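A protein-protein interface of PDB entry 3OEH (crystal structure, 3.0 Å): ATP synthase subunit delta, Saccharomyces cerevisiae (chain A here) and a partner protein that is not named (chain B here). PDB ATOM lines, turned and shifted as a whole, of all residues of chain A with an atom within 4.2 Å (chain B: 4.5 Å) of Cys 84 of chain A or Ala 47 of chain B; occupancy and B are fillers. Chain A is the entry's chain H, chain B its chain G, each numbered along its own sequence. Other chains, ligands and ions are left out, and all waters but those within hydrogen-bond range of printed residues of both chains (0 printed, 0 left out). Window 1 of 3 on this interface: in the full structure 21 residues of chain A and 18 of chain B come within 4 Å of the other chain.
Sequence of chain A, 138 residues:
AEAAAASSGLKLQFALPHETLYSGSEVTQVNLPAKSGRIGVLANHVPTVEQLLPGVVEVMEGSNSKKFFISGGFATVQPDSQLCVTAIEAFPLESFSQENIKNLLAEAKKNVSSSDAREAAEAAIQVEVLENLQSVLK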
ATOM      1  N   GLN A  13      10.385 -36.587  -0.312  1.00  0.00           N
ATOM      2  CA  GLN A  13       9.939 -35.373  -0.994  1.00  0.00           C
ATOM      3  C   GLN A  13      10.907 -34.900  -2.082  1.00  0.00           C
ATOM      4  O   GLN A  13      11.733 -34.006  -1.847  1.00  0.00           O
ATOM      5  CB  GLN A  13       9.699 -34.253   0.012  1.00  0.00           C
ATOM      6  CG  GLN A  13       8.240 -33.914   0.227  1.00  0.00           C
ATOM      7  CD  GLN A  13       8.063 -32.570   0.908  1.00  0.00           C
ATOM      8  OE1 GLN A  13       8.292 -32.436   2.117  1.00  0.00           O
ATOM      9  NE2 GLN A  13       7.656 -31.559   0.134  1.00  0.00           N
ATOM     10  N   PHE A  74      19.992 -29.718  -3.633  1.00  0.00           N
ATOM     11  CA  PHE A  74      20.198 -29.966  -2.217  1.00  0.00           C
ATOM     12  C   PHE A  74      19.316 -31.092  -1.716  1.00  0.00           C
ATOM     13  O   PHE A  74      18.139 -31.174  -2.067  1.00  0.00           O
ATOM     14  CB  PHE A  74      19.867 -28.710  -1.413  1.00  0.00           C
ATOM     15  CG  PHE A  74      21.053 -27.853  -1.098  1.00  0.00           C
ATOM     16  CD1 PHE A  74      21.455 -26.849  -1.970  1.00  0.00           C
ATOM     17  CD2 PHE A  74      21.754 -28.030   0.090  1.00  0.00           C
ATOM     18  CE1 PHE A  74      22.553 -26.038  -1.673  1.00  0.00           C
ATOM     19  CE2 PHE A  74      22.850 -27.222   0.405  1.00  0.00           C
ATOM     20  CZ  PHE A  74      23.250 -26.221  -0.482  1.00  0.00           C
ATOM     21  N   ALA A  75      19.901 -31.952  -0.887  1.00  0.00           N
ATOM     22  CA  ALA A  75      19.150 -32.949  -0.141  1.00  0.00           C
ATOM     23  C   ALA A  75      19.225 -32.620   1.340  1.00  0.00           C
ATOM     24  O   ALA A  75      20.263 -32.179   1.840  1.00  0.00           O
ATOM     25  CB  ALA A  75      19.689 -34.332  -0.402  1.00  0.00           C
ATOM     26  N   THR A  76      18.104 -32.796   2.028  1.00  0.00           N
ATOM     27  CA  THR A  76      18.078 -32.685   3.479  1.00  0.00           C
ATOM     28  C   THR A  76      17.213 -33.789   4.071  1.00  0.00           C
ATOM     29  O   THR A  76      16.109 -34.036   3.598  1.00  0.00           O
ATOM     30  CB  THR A  76      17.575 -31.291   3.999  1.00  0.00           C
ATOM     31  OG1 THR A  76      16.148 -31.213   3.898  1.00  0.00           O
ATOM     32  CG2 THR A  76      18.208 -30.130   3.234  1.00  0.00           C
ATOM     33  N   GLN A  78      15.198 -34.510   7.439  1.00  0.00           N
ATOM     34  CA  GLN A  78      14.638 -33.718   8.539  1.00  0.00           C
ATOM     35  C   GLN A  78      14.686 -34.434   9.899  1.00  0.00           C
ATOM     36  O   GLN A  78      15.032 -35.619   9.971  1.00  0.00           O
ATOM     37  CB  GLN A  78      13.200 -33.292   8.212  1.00  0.00           C
ATOM     38  CG  GLN A  78      13.015 -32.573   6.865  1.00  0.00           C
ATOM     39  CD  GLN A  78      13.709 -31.222   6.789  1.00  0.00           C
ATOM     40  OE1 GLN A  78      14.593 -30.912   7.588  1.00  0.00           O
ATOM     41  NE2 GLN A  78      13.318 -30.414   5.812  1.00  0.00           N
ATOM     42  N   GLN A  82      12.088 -37.394   7.290  1.00  0.00           N
ATOM     43  CA  GLN A  82      11.731 -37.208   5.881  1.00  0.00           C
ATOM     44  C   GLN A  82      12.920 -36.694   5.077  1.00  0.00           C
ATOM     45  O   GLN A  82      13.708 -35.884   5.571  1.00  0.00           O
ATOM     46  CB  GLN A  82      10.547 -36.244   5.733  1.00  0.00           C
ATOM     47  N   LEU A  83      13.052 -37.185   3.850  1.00  0.00           N
ATOM     48  CA  LEU A  83      14.068 -36.686   2.938  1.00  0.00           C
ATOM     49  C   LEU A  83      13.452 -35.646   2.014  1.00  0.00           C
ATOM     50  O   LEU A  83      12.362 -35.847   1.476  1.00  0.00           O
ATOM     51  CB  LEU A  83      14.699 -37.832   2.137  1.00  0.00           C
ATOM     52  CG  LEU A  83      15.826 -37.546   1.133  1.00  0.00           C
ATOM     53  CD1 LEU A  83      16.988 -36.765   1.736  1.00  0.00           C
ATOM     54  CD2 LEU A  83      16.327 -38.851   0.549  1.00  0.00           C
ATOM     55  N   CYS A  84      14.148 -34.528   1.855  1.00  0.00           N
ATOM     56  CA  CYS A  84      13.727 -33.475   0.943  1.00  0.00           C
ATOM     57  C   CYS A  84      14.798 -33.294  -0.110  1.00  0.00           C
ATOM     58  O   CYS A  84      15.933 -32.910   0.198  1.00  0.00           O
ATOM     59  CB  CYS A  84      13.489 -32.162   1.691  1.00  0.00           C
ATOM     60  SG  CYS A  84      12.218 -32.263   2.971  1.00  0.00           S
ATOM     61  N   VAL A  85      14.432 -33.589  -1.350  1.00  0.00           N
ATOM     62  CA  VAL A  85      15.341 -33.465  -2.478  1.00  0.00           C
ATOM     63  C   VAL A  85      14.819 -32.376  -3.408  1.00  0.00           C
ATOM     64  O   VAL A  85      13.622 -32.312  -3.691  1.00  0.00           O
ATOM     65  CB  VAL A  85      15.503 -34.823  -3.209  1.00  0.00           C
ATOM     66  CG1 VAL A  85      16.243 -34.668  -4.531  1.00  0.00           C
ATOM     67  CG2 VAL A  85      16.220 -35.814  -2.308  1.00  0.00           C
ATOM     68  N   LYS B  43       4.949 -26.401  -4.235  1.00  0.00           N
ATOM     69  CA  LYS B  43       5.310 -27.705  -3.671  1.00  0.00           C
ATOM     70  C   LYS B  43       6.792 -27.735  -3.303  1.00  0.00           C
ATOM     71  O   LYS B  43       7.167 -28.290  -2.272  1.00  0.00           O
ATOM     72  CB  LYS B  43       5.008 -28.825  -4.672  1.00  0.00           C
ATOM     73  CG  LYS B  43       4.655 -30.162  -4.046  1.00  0.00           C
ATOM     74  CD  LYS B  43       3.168 -30.236  -3.698  1.00  0.00           C
ATOM     75  CE  LYS B  43       2.836 -31.478  -2.883  1.00  0.00           C
ATOM     76  NZ  LYS B  43       3.500 -31.463  -1.544  1.00  0.00           N
ATOM     77  N   MET B  44       7.619 -27.123  -4.146  1.00  0.00           N
ATOM     78  CA  MET B  44       9.062 -27.092  -3.939  1.00  0.00           C
ATOM     79  C   MET B  44       9.478 -26.148  -2.812  1.00  0.00           C
ATOM     80  O   MET B  44      10.604 -26.238  -2.306  1.00  0.00           O
ATOM     81  CB  MET B  44       9.776 -26.691  -5.224  1.00  0.00           C
ATOM     82  CG  MET B  44      11.214 -27.130  -5.276  1.00  0.00           C
ATOM     83  SD  MET B  44      12.176 -25.954  -6.211  1.00  0.00           S
ATOM     84  CE  MET B  44      13.522 -27.009  -6.738  1.00  0.00           C
ATOM     85  N   ASP B  45       8.584 -25.240  -2.425  1.00  0.00           N
ATOM     86  CA  ASP B  45       8.886 -24.342  -1.317  1.00  0.00           C
ATOM     87  C   ASP B  45       8.860 -25.068   0.028  1.00  0.00           C
ATOM     88  O   ASP B  45       9.791 -24.931   0.829  1.00  0.00           O
ATOM     89  CB  ASP B  45       7.978 -23.107  -1.298  1.00  0.00           C
ATOM     90  CG  ASP B  45       8.615 -21.939  -0.543  1.00  0.00           C
ATOM     91  OD1 ASP B  45       9.731 -21.506  -0.944  1.00  0.00           O
ATOM     92  OD2 ASP B  45       8.012 -21.468   0.453  1.00  0.00           O
ATOM     93  N   GLU B  46       7.804 -25.852   0.257  1.00  0.00           N
ATOM     94  CA  GLU B  46       7.642 -26.612   1.501  1.00  0.00           C
ATOM     95  C   GLU B  46       8.865 -27.476   1.764  1.00  0.00           C
ATOM     96  O   GLU B  46       9.305 -27.583   2.900  1.00  0.00           O
ATOM     97  CB  GLU B  46       6.375 -27.490   1.486  1.00  0.00           C
ATOM     98  CG  GLU B  46       5.201 -27.032   0.585  1.00  0.00           C
ATOM     99  CD  GLU B  46       4.724 -25.587   0.822  1.00  0.00           C
ATOM    100  OE1 GLU B  46       5.255 -24.899   1.731  1.00  0.00           O
ATOM    101  OE2 GLU B  46       3.811 -25.138   0.081  1.00  0.00           O
ATOM    102  N   ALA B  47       9.414 -28.069   0.705  1.00  0.00           N
ATOM    103  CA  ALA B  47      10.571 -28.967   0.807  1.00  0.00           C
ATOM    104  C   ALA B  47      11.888 -28.233   1.067  1.00  0.00           C
ATOM    105  O   ALA B  47      12.766 -28.744   1.760  1.00  0.00           O
ATOM    106  CB  ALA B  47      10.683 -29.836  -0.450  1.00  0.00           C
ATOM    107  N   GLU B  48      12.023 -27.037   0.506  1.00  0.00           N
ATOM    108  CA  GLU B  48      13.242 -26.255   0.663  1.00  0.00           C
ATOM    109  C   GLU B  48      13.233 -25.384   1.922  1.00  0.00           C
ATOM    110  O   GLU B  48      14.236 -25.300   2.630  1.00  0.00           O
ATOM    111  CB  GLU B  48      13.488 -25.407  -0.586  1.00  0.00           C
ATOM    112  CG  GLU B  48      13.795 -23.952  -0.297  1.00  0.00           C
ATOM    113  CD  GLU B  48      14.773 -23.364  -1.274  1.00  0.00           C
ATOM    114  OE1 GLU B  48      15.937 -23.832  -1.301  1.00  0.00           O
ATOM    115  OE2 GLU B  48      14.378 -22.427  -2.005  1.00  0.00           O
ATOM    116  N   GLN B  49      12.095 -24.740   2.176  1.00  0.00           N
ATOM    117  CA  GLN B  49      11.930 -23.825   3.307  1.00  0.00           C
ATOM    118  C   GLN B  49      11.563 -24.556   4.596  1.00  0.00           C
ATOM    119  O   GLN B  49      11.338 -23.920   5.627  1.00  0.00           O
ATOM    120  CB  GLN B  49      10.886 -22.736   2.984  1.00  0.00           C
ATOM    121  CG  GLN B  49      11.471 -21.376   2.555  1.00  0.00           C
ATOM    122  CD  GLN B  49      11.497 -20.338   3.686  1.00  0.00           C
ATOM    123  OE1 GLN B  49      10.995 -20.583   4.789  1.00  0.00           O
ATOM    124  NE2 GLN B  49      12.074 -19.167   3.406  1.00  0.00           N
ATOM    125  N   LEU B  50      11.498 -25.885   4.532  1.00  0.00           N
ATOM    126  CA  LEU B  50      11.279 -26.708   5.720  1.00  0.00           C
ATOM    127  C   LEU B  50      12.545 -26.783   6.564  1.00  0.00           C
ATOM    128  O   LEU B  50      12.474 -26.664   7.784  1.00  0.00           O
ATOM    129  CB  LEU B  50      10.798 -28.118   5.348  1.00  0.00           C
ATOM    130  CG  LEU B  50      10.418 -29.098   6.467  1.00  0.00           C
ATOM    131  CD1 LEU B  50       9.396 -28.496   7.424  1.00  0.00           C
ATOM    132  CD2 LEU B  50       9.907 -30.410   5.884  1.00  0.00           C
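The backbone carbonyl oxygen of Ala 47 of chain B sits close to the side-chain sulfur of Cys 84 of chain A (3.8 Å).
The backbone carbonyl oxygen of Leu 83 of chain A lies within hydrogen-bond range of the backbone NH of Gln 13 of chain A (2.8 Å). The backbone carbonyl oxygen of Gln 13 of chain A lies within hydrogen-bond range of the backbone NH of Val 85 of chain A, at 2.8 Å. The backbone NH (N) of Cys 84 of chain A lies within hydrogen-bond range of the backbone carbonyl oxygen (O) of Thr 76 of chain A. SG of Cys 84 of chain A lies within hydrogen-bond range of NE2 of Gln 78 of chain A, at 3.6 Å.
Gln 13 of chain A touches Ala 47 of chain B (NE2 to CB, 3.5 Å). NE2 of Gln 78 of chain A touches CG of Leu 50 of chain B, at 3.3 Å.
Of the printed residues of chain B, Gln 13 of chain A touches Ala 47. Phe 74 of chain A touches none of the printed residues of chain B. Printed residues of chain B within 4 Å of Gln 78 of chain A: Leu 50. Ala 47 of chain B touches just these residues of chain A: Gln 13 and Cys 84. Printed residues of chain A within 4 Å of Leu 50 of chain B: Gln 78 (3.3 Å).
Of the 9 printed residues of chain A, 3 touch a printed residue of chain B. Of the 8 printed residues of chain B, 2 touch a printed residue of chain A. Printed residues of chain B that touch a printed residue of chain A: Ala 47 and Leu 50. Hydrophobic or aromatic side chains of chain B within 4 Å of the printed part of chain A: Ala 47 and Leu 50. Among the printed residues, 3 pairs touch across the chains. Among the printed residues, no Asp or Glu carboxylate lies within 4 Å of a Lys or Arg side-chain nitrogen of the other chain.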
